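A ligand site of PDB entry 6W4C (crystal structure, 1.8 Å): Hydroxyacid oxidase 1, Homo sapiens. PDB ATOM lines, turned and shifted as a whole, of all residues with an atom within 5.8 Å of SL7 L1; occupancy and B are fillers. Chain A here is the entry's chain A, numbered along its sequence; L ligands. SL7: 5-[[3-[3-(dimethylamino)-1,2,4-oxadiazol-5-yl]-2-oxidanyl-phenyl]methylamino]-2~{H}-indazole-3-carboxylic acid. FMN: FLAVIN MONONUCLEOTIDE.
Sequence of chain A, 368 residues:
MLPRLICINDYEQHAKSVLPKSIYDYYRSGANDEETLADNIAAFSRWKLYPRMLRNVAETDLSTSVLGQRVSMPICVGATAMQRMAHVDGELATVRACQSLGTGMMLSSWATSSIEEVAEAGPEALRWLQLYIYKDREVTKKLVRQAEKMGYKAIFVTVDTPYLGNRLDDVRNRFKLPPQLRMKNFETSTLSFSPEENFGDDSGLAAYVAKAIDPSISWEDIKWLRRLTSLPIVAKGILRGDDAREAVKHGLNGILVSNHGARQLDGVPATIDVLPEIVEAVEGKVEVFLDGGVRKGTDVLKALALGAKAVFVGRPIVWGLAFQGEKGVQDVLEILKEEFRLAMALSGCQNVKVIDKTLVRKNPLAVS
The side-chain hydroxyl of Tyr 132 sits at hydrogen-bond distance from a nitrogen (N4) of SL7 L1 (2.6 Å). An oxygen (O1) of SL7 L1 is in hydrogen-bond range of the side-chain hydroxyl (OH) of Tyr 26, 2.7 Å away. A nitrogen (N5) of SL7 L1 lies within hydrogen-bond range of a ring nitrogen (NE2) of His 260 (2.8 Å). The guanidinium group of Arg 263 is in salt-bridge range of an oxygen (O2) of SL7 L1 (2.8 Å). An oxygen (O2) of SL7 L1 is in salt-bridge range of the guanidinium group (NH2) of Arg 167 (2.9 Å). OH of Tyr 132 is in hydrogen-bond range of N3 of FMN L2 (3.4 Å). N of Ala 81 lies within hydrogen-bond range of N5 of FMN L2, at 3.1 Å. O4 of FMN L2 lies within hydrogen-bond range of OG of Ser 108.
N5 of SL7 L1 lies close to N5 of FMN L2.
The guanidinium group (NH1) of Arg 263 is in hydrogen-bond range of the backbone carbonyl oxygen (O) of Tyr 26 (2.8 Å). ND1 of His 260 is in hydrogen-bond range of OG1 of Thr 161, at 3.4 Å. The guanidinium group of Arg 167 lies within hydrogen-bond range of the backbone carbonyl oxygen of Arg 263. OE1 of Gln 264 is in hydrogen-bond range of NH2 of Arg 167 (3.2 Å). The backbone carbonyl oxygen of Trp 110 lies within hydrogen-bond range of the backbone NH of Met 82 (3.2 Å). The side-chain hydroxyl (OG) of Ser 108 sits at hydrogen-bond distance from the backbone NH (N) of Trp 110, at 3.0 Å.
O of Arg 174 lies close to N1 of SL7 L1 (3.4 Å). Residues that only touch SL7 L1: Met 82, Met 85, Trp 110, Phe 175, Ala 206, Ala 81, Gly 204, Ser 22, Val 209 and Asp 170. Hydrophobic or aromatic side chains within 4 Å of SL7 L1: Tyr 26, Ala 81, Met 82, Met 85, Trp 110, Tyr 132, Phe 175, Ala 206, Val 209 and His 260. 16 residues have an atom within 4 Å of SL7 L1: Ser 22, Tyr 26, Ala 81, Met 82, Met 85, Trp 110, Tyr 132, Arg 167, Asp 170, Arg 174, Phe 175, Gly 204, Ala 206, Val 209, His 260 and Arg 263. Along chain A the residues within 4 Å of SL7 L1 span positions 22 to 263. The nearest printed residue that does not touch SL7 L1 is Ile 23 (4.4 Å).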
ATOM      1  N   SER A  22      34.204 -26.793 -16.562  1.00  0.00           N
ATOM      2  CA  SER A  22      32.814 -26.398 -16.176  1.00  0.00           C
ATOM      3  C   SER A  22      32.537 -26.830 -14.726  1.00  0.00           C
ATOM      4  O   SER A  22      31.892 -26.040 -14.003  1.00  0.00           O
ATOM      5  CB  SER A  22      31.798 -26.942 -17.141  1.00  0.00           C
ATOM      6  OG  SER A  22      31.636 -28.347 -16.981  1.00  0.00           O
ATOM      7  N   ILE A  23      33.037 -27.994 -14.304  1.00  0.00           N
ATOM      8  CA  ILE A  23      32.819 -28.558 -12.938  1.00  0.00           C
ATOM      9  C   ILE A  23      33.697 -27.773 -11.959  1.00  0.00           C
ATOM     10  O   ILE A  23      33.174 -27.351 -10.905  1.00  0.00           O
ATOM     11  CB  ILE A  23      33.121 -30.068 -12.880  1.00  0.00           C
ATOM     12  CG1 ILE A  23      32.239 -30.847 -13.864  1.00  0.00           C
ATOM     13  CG2 ILE A  23      33.001 -30.586 -11.459  1.00  0.00           C
ATOM     14  CD1 ILE A  23      32.371 -32.358 -13.771  1.00  0.00           C
ATOM     15  N   TYR A  26      32.145 -24.357 -11.505  1.00  0.00           N
ATOM     16  CA  TYR A  26      30.924 -24.472 -10.665  1.00  0.00           C
ATOM     17  C   TYR A  26      31.340 -24.447  -9.180  1.00  0.00           C
ATOM     18  O   TYR A  26      30.730 -23.684  -8.377  1.00  0.00           O
ATOM     19  CB  TYR A  26      30.108 -25.725 -10.954  1.00  0.00           C
ATOM     20  CG  TYR A  26      29.128 -26.034  -9.850  1.00  0.00           C
ATOM     21  CD1 TYR A  26      28.024 -25.216  -9.642  1.00  0.00           C
ATOM     22  CD2 TYR A  26      29.322 -27.084  -8.977  1.00  0.00           C
ATOM     23  CE1 TYR A  26      27.136 -25.456  -8.608  1.00  0.00           C
ATOM     24  CE2 TYR A  26      28.434 -27.341  -7.946  1.00  0.00           C
ATOM     25  CZ  TYR A  26      27.359 -26.511  -7.744  1.00  0.00           C
ATOM     26  OH  TYR A  26      26.491 -26.745  -6.717  1.00  0.00           O
ATOM     27  N   ALA A  81      26.293 -29.380  -2.413  1.00  0.00           N
ATOM     28  CA  ALA A  81      25.360 -30.155  -3.251  1.00  0.00           C
ATOM     29  C   ALA A  81      26.153 -31.086  -4.186  1.00  0.00           C
ATOM     30  O   ALA A  81      27.254 -30.698  -4.605  1.00  0.00           O
ATOM     31  CB  ALA A  81      24.485 -29.215  -4.037  1.00  0.00           C
ATOM     32  N   MET A  82      25.593 -32.277  -4.431  1.00  0.00           N
ATOM     33  CA  MET A  82      25.950 -33.220  -5.530  1.00  0.00           C
ATOM     34  C   MET A  82      27.459 -33.453  -5.597  1.00  0.00           C
ATOM     35  O   MET A  82      28.117 -33.107  -6.596  1.00  0.00           O
ATOM     36  CB  MET A  82      25.445 -32.677  -6.864  1.00  0.00           C
ATOM     37  CG  MET A  82      23.983 -32.280  -6.806  1.00  0.00           C
ATOM     38  SD  MET A  82      23.366 -31.824  -8.425  1.00  0.00           S
ATOM     39  CE  MET A  82      24.742 -30.867  -9.046  1.00  0.00           C
ATOM     40  N   MET A  85      29.688 -35.421  -8.432  1.00  0.00           N
ATOM     41  CA  MET A  85      30.349 -34.755  -9.581  1.00  0.00           C
ATOM     42  C   MET A  85      31.865 -34.739  -9.401  1.00  0.00           C
ATOM     43  O   MET A  85      32.579 -34.710 -10.410  1.00  0.00           O
ATOM     44  CB  MET A  85      29.867 -33.308  -9.723  1.00  0.00           C
ATOM     45  CG  MET A  85      28.504 -33.178 -10.307  1.00  0.00           C
ATOM     46  SD  MET A  85      28.315 -31.524 -11.019  1.00  0.00           S
ATOM     47  CE  MET A  85      29.584 -31.593 -12.276  1.00  0.00           C
ATOM     48  N   SER A 108      24.008 -31.954   2.467  1.00  0.00           N
ATOM     49  CA  SER A 108      23.154 -31.092   1.622  1.00  0.00           C
ATOM     50  C   SER A 108      21.788 -31.767   1.431  1.00  0.00           C
ATOM     51  O   SER A 108      21.768 -32.984   1.282  1.00  0.00           O
ATOM     52  CB  SER A 108      23.825 -30.836   0.311  1.00  0.00           C
ATOM     53  OG  SER A 108      22.957 -30.165  -0.582  1.00  0.00           O
ATOM     54  N   TRP A 110      20.263 -31.328  -1.162  1.00  0.00           N
ATOM     55  CA  TRP A 110      20.387 -31.607  -2.620  1.00  0.00           C
ATOM     56  C   TRP A 110      21.622 -32.490  -2.881  1.00  0.00           C
ATOM     57  O   TRP A 110      22.509 -32.082  -3.640  1.00  0.00           O
ATOM     58  CB  TRP A 110      20.380 -30.304  -3.426  1.00  0.00           C
ATOM     59  CG  TRP A 110      19.775 -30.514  -4.770  1.00  0.00           C
ATOM     60  CD1 TRP A 110      20.351 -31.121  -5.846  1.00  0.00           C
ATOM     61  CD2 TRP A 110      18.440 -30.177  -5.174  1.00  0.00           C
ATOM     62  NE1 TRP A 110      19.475 -31.159  -6.904  1.00  0.00           N
ATOM     63  CE2 TRP A 110      18.288 -30.599  -6.518  1.00  0.00           C
ATOM     64  CE3 TRP A 110      17.358 -29.553  -4.543  1.00  0.00           C
ATOM     65  CZ2 TRP A 110      17.109 -30.405  -7.227  1.00  0.00           C
ATOM     66  CZ3 TRP A 110      16.183 -29.366  -5.246  1.00  0.00           C
ATOM     67  CH2 TRP A 110      16.057 -29.791  -6.577  1.00  0.00           C
ATOM     68  N   TYR A 132      16.563 -26.943   2.935  1.00  0.00           N
ATOM     69  CA  TYR A 132      15.802 -25.818   2.343  1.00  0.00           C
ATOM     70  C   TYR A 132      14.331 -26.072   2.657  1.00  0.00           C
ATOM     71  O   TYR A 132      13.931 -27.252   2.587  1.00  0.00           O
ATOM     72  CB  TYR A 132      16.005 -25.721   0.835  1.00  0.00           C
ATOM     73  CG  TYR A 132      17.377 -25.255   0.434  1.00  0.00           C
ATOM     74  CD1 TYR A 132      17.750 -23.945   0.665  1.00  0.00           C
ATOM     75  CD2 TYR A 132      18.279 -26.101  -0.181  1.00  0.00           C
ATOM     76  CE1 TYR A 132      19.002 -23.483   0.297  1.00  0.00           C
ATOM     77  CE2 TYR A 132      19.546 -25.661  -0.554  1.00  0.00           C
ATOM     78  CZ  TYR A 132      19.904 -24.348  -0.307  1.00  0.00           C
ATOM     79  OH  TYR A 132      21.132 -23.870  -0.657  1.00  0.00           O
ATOM     80  N   THR A 161      18.793 -18.053   0.748  1.00  0.00           N
ATOM     81  CA  THR A 161      18.586 -18.547  -0.643  1.00  0.00           C
ATOM     82  C   THR A 161      17.103 -18.539  -0.993  1.00  0.00           C
ATOM     83  O   THR A 161      16.523 -19.583  -1.304  1.00  0.00           O
ATOM     84  CB  THR A 161      19.248 -19.918  -0.819  1.00  0.00           C
ATOM     85  OG1 THR A 161      20.564 -19.864  -0.271  1.00  0.00           O
ATOM     86  CG2 THR A 161      19.374 -20.345  -2.268  1.00  0.00           C
ATOM     87  N   LEU A 164      18.527 -18.540  -6.178  1.00  0.00           N
ATOM     88  CA  LEU A 164      19.968 -18.855  -6.365  1.00  0.00           C
ATOM     89  C   LEU A 164      20.722 -17.612  -6.859  1.00  0.00           C
ATOM     90  O   LEU A 164      20.197 -16.864  -7.701  1.00  0.00           O
ATOM     91  CB  LEU A 164      20.113 -20.018  -7.352  1.00  0.00           C
ATOM     92  CG  LEU A 164      20.025 -21.409  -6.725  1.00  0.00           C
ATOM     93  CD1 LEU A 164      21.207 -21.705  -5.811  1.00  0.00           C
ATOM     94  CD2 LEU A 164      18.718 -21.584  -5.964  1.00  0.00           C
ATOM     95  N   ARG A 167      25.994 -16.756 -10.559  1.00  0.00           N
ATOM     96  CA  ARG A 167      27.421 -17.123 -10.747  1.00  0.00           C
ATOM     97  C   ARG A 167      27.671 -17.131 -12.262  1.00  0.00           C
ATOM     98  O   ARG A 167      27.053 -17.962 -12.964  1.00  0.00           O
ATOM     99  CB  ARG A 167      27.735 -18.441 -10.029  1.00  0.00           C
ATOM    100  CG  ARG A 167      27.332 -18.469  -8.551  1.00  0.00           C
ATOM    101  CD  ARG A 167      25.971 -19.124  -8.371  1.00  0.00           C
ATOM    102  NE  ARG A 167      25.472 -19.285  -6.985  1.00  0.00           N
ATOM    103  CZ  ARG A 167      25.327 -20.448  -6.350  1.00  0.00           C
ATOM    104  NH1 ARG A 167      25.689 -21.568  -6.957  1.00  0.00           N
ATOM    105  NH2 ARG A 167      24.835 -20.476  -5.120  1.00  0.00           N
ATOM    106  N   ASP A 170      28.752 -20.291 -14.478  1.00  0.00           N
ATOM    107  CA  ASP A 170      27.673 -21.311 -14.621  1.00  0.00           C
ATOM    108  C   ASP A 170      26.764 -20.907 -15.777  1.00  0.00           C
ATOM    109  O   ASP A 170      26.307 -21.812 -16.514  1.00  0.00           O
ATOM    110  CB  ASP A 170      26.858 -21.475 -13.338  1.00  0.00           C
ATOM    111  CG  ASP A 170      27.646 -22.059 -12.174  1.00  0.00           C
ATOM    112  OD1 ASP A 170      28.827 -22.431 -12.396  1.00  0.00           O
ATOM    113  OD2 ASP A 170      27.088 -22.135 -11.058  1.00  0.00           O
ATOM    114  N   ASN A 173      28.712 -21.568 -19.053  1.00  0.00           N
ATOM    115  CA  ASN A 173      28.871 -23.024 -19.296  1.00  0.00           C
ATOM    116  C   ASN A 173      27.511 -23.744 -19.338  1.00  0.00           C
ATOM    117  O   ASN A 173      27.515 -24.971 -19.568  1.00  0.00           O
ATOM    118  CB  ASN A 173      29.758 -23.691 -18.237  1.00  0.00           C
ATOM    119  CG  ASN A 173      31.095 -23.009 -18.051  1.00  0.00           C
ATOM    120  OD1 ASN A 173      31.615 -22.376 -18.963  1.00  0.00           O
ATOM    121  ND2 ASN A 173      31.667 -23.128 -16.858  1.00  0.00           N
ATOM    122  N   ARG A 174      26.397 -23.038 -19.122  1.00  0.00           N
ATOM    123  CA  ARG A 174      25.041 -23.629 -18.938  1.00  0.00           C
ATOM    124  C   ARG A 174      25.095 -24.613 -17.760  1.00  0.00           C
ATOM    125  O   ARG A 174      25.689 -24.259 -16.719  1.00  0.00           O
ATOM    126  CB  ARG A 174      24.561 -24.285 -20.240  1.00  0.00           C
ATOM    127  CG  ARG A 174      24.932 -23.545 -21.522  1.00  0.00           C
ATOM    128  CD  ARG A 174      24.097 -22.313 -21.790  1.00  0.00           C
ATOM    129  NE  ARG A 174      24.127 -22.004 -23.209  1.00  0.00           N
ATOM    130  CZ  ARG A 174      23.465 -22.665 -24.159  1.00  0.00           C
ATOM    131  NH1 ARG A 174      22.688 -23.688 -23.847  1.00  0.00           N
ATOM    132  NH2 ARG A 174      23.597 -22.311 -25.423  1.00  0.00           N
ATOM    133  N   PHE A 175      24.495 -25.811 -17.897  1.00  0.00           N
ATOM    134  CA  PHE A 175      24.550 -26.919 -16.907  1.00  0.00           C
ATOM    135  C   PHE A 175      24.858 -28.235 -17.627  1.00  0.00           C
ATOM    136  O   PHE A 175      25.999 -28.369 -18.121  1.00  0.00           O
ATOM    137  CB  PHE A 175      23.233 -27.009 -16.123  1.00  0.00           C
ATOM    138  CG  PHE A 175      22.504 -25.700 -15.956  1.00  0.00           C
ATOM    139  CD1 PHE A 175      22.980 -24.731 -15.086  1.00  0.00           C
ATOM    140  CD2 PHE A 175      21.354 -25.440 -16.676  1.00  0.00           C
ATOM    141  CE1 PHE A 175      22.301 -23.532 -14.934  1.00  0.00           C
ATOM    142  CE2 PHE A 175      20.684 -24.235 -16.523  1.00  0.00           C
ATOM    143  CZ  PHE A 175      21.159 -23.283 -15.657  1.00  0.00           C
ATOM    144  N   GLY A 204      19.782 -30.616 -10.364  1.00  0.00           N
ATOM    145  CA  GLY A 204      21.023 -30.773 -11.168  1.00  0.00           C
ATOM    146  C   GLY A 204      21.242 -29.594 -12.099  1.00  0.00           C
ATOM    147  O   GLY A 204      22.383 -29.109 -12.185  1.00  0.00           O
ATOM    148  N   LEU A 205      20.174 -29.172 -12.785  1.00  0.00           N
ATOM    149  CA  LEU A 205      20.094 -27.907 -13.565  1.00  0.00           C
ATOM    150  C   LEU A 205      19.582 -26.820 -12.628  1.00  0.00           C
ATOM    151  O   LEU A 205      18.688 -27.134 -11.801  1.00  0.00           O
ATOM    152  CB  LEU A 205      19.160 -28.094 -14.764  1.00  0.00           C
ATOM    153  CG  LEU A 205      19.491 -29.253 -15.707  1.00  0.00           C
ATOM    154  CD1 LEU A 205      18.974 -30.585 -15.181  1.00  0.00           C
ATOM    155  CD2 LEU A 205      18.917 -28.997 -17.098  1.00  0.00           C
ATOM    156  N   ALA A 206      20.111 -25.593 -12.734  1.00  0.00           N
ATOM    157  CA  ALA A 206      19.667 -24.428 -11.943  1.00  0.00           C
ATOM    158  C   ALA A 206      18.162 -24.238 -12.158  1.00  0.00           C
ATOM    159  O   ALA A 206      17.462 -23.867 -11.192  1.00  0.00           O
ATOM    160  CB  ALA A 206      20.442 -23.196 -12.311  1.00  0.00           C
ATOM    161  N   VAL A 209      16.264 -26.658  -9.740  1.00  0.00           N
ATOM    162  CA  VAL A 209      16.525 -26.228  -8.327  1.00  0.00           C
ATOM    163  C   VAL A 209      15.763 -24.917  -8.065  1.00  0.00           C
ATOM    164  O   VAL A 209      15.132 -24.807  -6.999  1.00  0.00           O
ATOM    165  CB  VAL A 209      18.032 -26.071  -8.020  1.00  0.00           C
ATOM    166  CG1 VAL A 209      18.278 -25.488  -6.636  1.00  0.00           C
ATOM    167  CG2 VAL A 209      18.774 -27.381  -8.181  1.00  0.00           C
ATOM    168  N   HIS A 260      27.203 -18.177   2.290  1.00  0.00           N
ATOM    169  CA  HIS A 260      27.002 -19.273   1.307  1.00  0.00           C
ATOM    170  C   HIS A 260      28.258 -19.389   0.438  1.00  0.00           C
ATOM    171  O   HIS A 260      28.124 -19.562  -0.790  1.00  0.00           O
ATOM    172  CB  HIS A 260      25.752 -18.992   0.458  1.00  0.00           C
ATOM    173  CG  HIS A 260      25.085 -20.201  -0.095  1.00  0.00           C
ATOM    174  ND1 HIS A 260      23.838 -20.606   0.341  1.00  0.00           N
ATOM    175  CD2 HIS A 260      25.453 -21.086  -1.062  1.00  0.00           C
ATOM    176  CE1 HIS A 260      23.466 -21.682  -0.337  1.00  0.00           C
ATOM    177  NE2 HIS A 260      24.441 -21.991  -1.201  1.00  0.00           N
ATOM    178  N   ARG A 263      28.449 -17.079  -2.745  1.00  0.00           N
ATOM    179  CA  ARG A 263      27.762 -17.543  -3.975  1.00  0.00           C
ATOM    180  C   ARG A 263      26.362 -16.942  -4.112  1.00  0.00           C
ATOM    181  O   ARG A 263      25.699 -17.213  -5.142  1.00  0.00           O
ATOM    182  CB  ARG A 263      27.704 -19.069  -3.934  1.00  0.00           C
ATOM    183  CG  ARG A 263      29.078 -19.714  -4.006  1.00  0.00           C
ATOM    184  CD  ARG A 263      29.055 -21.173  -3.631  1.00  0.00           C
ATOM    185  NE  ARG A 263      28.425 -22.060  -4.602  1.00  0.00           N
ATOM    186  CZ  ARG A 263      29.044 -22.588  -5.665  1.00  0.00           C
ATOM    187  NH1 ARG A 263      30.271 -22.240  -5.981  1.00  0.00           N
ATOM    188  NH2 ARG A 263      28.403 -23.447  -6.436  1.00  0.00           N
ATOM    189  N   GLN A 264      25.891 -16.175  -3.126  1.00  0.00           N
ATOM    190  CA  GLN A 264      24.510 -15.634  -3.160  1.00  0.00           C
ATOM    191  C   GLN A 264      24.571 -14.146  -3.510  1.00  0.00           C
ATOM    192  O   GLN A 264      24.660 -13.807  -4.710  1.00  0.00           O
ATOM    193  CB  GLN A 264      23.800 -15.977  -1.842  1.00  0.00           C
ATOM    194  CG  GLN A 264      23.412 -17.447  -1.771  1.00  0.00           C
ATOM    195  CD  GLN A 264      22.380 -17.775  -2.826  1.00  0.00           C
ATOM    196  OE1 GLN A 264      22.652 -18.480  -3.799  1.00  0.00           O
ATOM    197  NE2 GLN A 264      21.192 -17.204  -2.667  1.00  0.00           N
HETATM  198  C1  SL7 L   1      28.058 -28.753 -12.475  1.00  0.00           C
HETATM  199  C2  SL7 L   1      26.907 -26.693 -13.118  1.00  0.00           C
HETATM  200  C3  SL7 L   1      25.363 -25.995 -11.987  1.00  0.00           C
HETATM  201  C7  SL7 L   1      22.369 -25.847  -8.972  1.00  0.00           C
HETATM  202  C8  SL7 L   1      23.246 -26.924  -9.016  1.00  0.00           C
HETATM  203  C9  SL7 L   1      23.201 -28.079  -8.045  1.00  0.00           C
HETATM  204  C10 SL7 L   1      22.217 -27.224  -5.915  1.00  0.00           C
HETATM  205  C11 SL7 L   1      23.264 -26.305  -5.731  1.00  0.00           C
HETATM  206  C12 SL7 L   1      23.271 -25.516  -4.581  1.00  0.00           C
HETATM  207  C13 SL7 L   1      22.229 -25.658  -3.645  1.00  0.00           C
HETATM  208  C14 SL7 L   1      24.102 -24.478  -4.044  1.00  0.00           C
HETATM  209  C15 SL7 L   1      25.328 -23.851  -4.575  1.00  0.00           C
HETATM  210  C16 SL7 L   1      21.204 -26.574  -3.821  1.00  0.00           C
HETATM  211  O2  SL7 L   1      25.841 -22.903  -3.984  1.00  0.00           O
HETATM  212  O1  SL7 L   1      25.799 -24.349  -5.684  1.00  0.00           O
HETATM  213  N5  SL7 L   1      23.616 -24.036  -2.886  1.00  0.00           N
HETATM  214  N4  SL7 L   1      22.476 -24.758  -2.656  1.00  0.00           N
HETATM  215  C17 SL7 L   1      21.206 -27.340  -4.968  1.00  0.00           C
HETATM  216  N3  SL7 L   1      22.158 -28.028  -7.045  1.00  0.00           N
HETATM  217  C6  SL7 L   1      22.471 -24.805  -9.879  1.00  0.00           C
HETATM  218  C5  SL7 L   1      23.455 -24.805 -10.861  1.00  0.00           C
HETATM  219  C18 SL7 L   1      24.225 -26.935 -10.006  1.00  0.00           C
HETATM  220  O3  SL7 L   1      25.068 -27.981 -10.022  1.00  0.00           O
HETATM  221  C4  SL7 L   1      24.335 -25.882 -10.941  1.00  0.00           C
HETATM  222  O   SL7 L   1      25.631 -25.039 -12.896  1.00  0.00           O
HETATM  223  N1  SL7 L   1      26.708 -25.545 -13.692  1.00  0.00           N
HETATM  224  N2  SL7 L   1      26.124 -27.035 -12.092  1.00  0.00           N
HETATM  225  N   SL7 L   1      27.840 -27.627 -13.376  1.00  0.00           N
HETATM  226  C   SL7 L   1      28.697 -27.577 -14.552  1.00  0.00           C
HETATM  227  N1  FMN L   2      24.960 -24.569   1.222  1.00  0.00           N
HETATM  228  C2  FMN L   2      23.773 -25.154   1.514  1.00  0.00           C
HETATM  229  O2  FMN L   2      23.137 -24.759   2.532  1.00  0.00           O
HETATM  230  N3  FMN L   2      23.264 -26.161   0.761  1.00  0.00           N
HETATM  231  C4  FMN L   2      23.891 -26.627  -0.320  1.00  0.00           C
HETATM  232  O4  FMN L   2      23.432 -27.533  -1.020  1.00  0.00           O
HETATM  233  C4A FMN L   2      25.165 -26.014  -0.712  1.00  0.00           C
HETATM  234  N5  FMN L   2      25.834 -26.413  -1.811  1.00  0.00           N
HETATM  235  C5A FMN L   2      27.016 -25.874  -2.105  1.00  0.00           C
HETATM  236  C6  FMN L   2      27.724 -26.331  -3.216  1.00  0.00           C
HETATM  237  C7  FMN L   2      28.940 -25.770  -3.507  1.00  0.00           C
HETATM  238  C7M FMN L   2      29.705 -26.248  -4.704  1.00  0.00           C
HETATM  239  C8  FMN L   2      29.538 -24.708  -2.683  1.00  0.00           C
HETATM  240  C8M FMN L   2      30.895 -24.118  -3.025  1.00  0.00           C
HETATM  241  C9  FMN L   2      28.855 -24.254  -1.559  1.00  0.00           C
HETATM  242  C9A FMN L   2      27.600 -24.812  -1.251  1.00  0.00           C
HETATM  243  N10 FMN L   2      26.896 -24.362  -0.134  1.00  0.00           N
HETATM  244  C10 FMN L   2      25.680 -24.962   0.179  1.00  0.00           C
HETATM  245  C1' FMN L   2      27.423 -23.348   0.771  1.00  0.00           C
HETATM  246  C2' FMN L   2      28.305 -24.124   1.752  1.00  0.00           C
HETATM  247  O2' FMN L   2      27.526 -24.893   2.672  1.00  0.00           O
HETATM  248  C3' FMN L   2      29.193 -23.229   2.614  1.00  0.00           C
HETATM  249  O3' FMN L   2      28.428 -22.134   3.189  1.00  0.00           O
HETATM  250  C4' FMN L   2      30.360 -22.645   1.847  1.00  0.00           C
HETATM  251  O4' FMN L   2      30.941 -23.586   0.933  1.00  0.00           O
HETATM  252  C5' FMN L   2      31.435 -22.191   2.815  1.00  0.00           C
HETATM  253  O5' FMN L   2      32.513 -21.492   2.202  1.00  0.00           O
HETATM  254  P   FMN L   2      33.906 -22.170   1.728  1.00  0.00           P
HETATM  255  O1P FMN L   2      34.393 -23.123   2.801  1.00  0.00           O
HETATM  256  O2P FMN L   2      33.561 -22.944   0.478  1.00  0.00           O
HETATM  257  O3P FMN L   2      34.792 -20.972   1.465  1.00  0.00           O
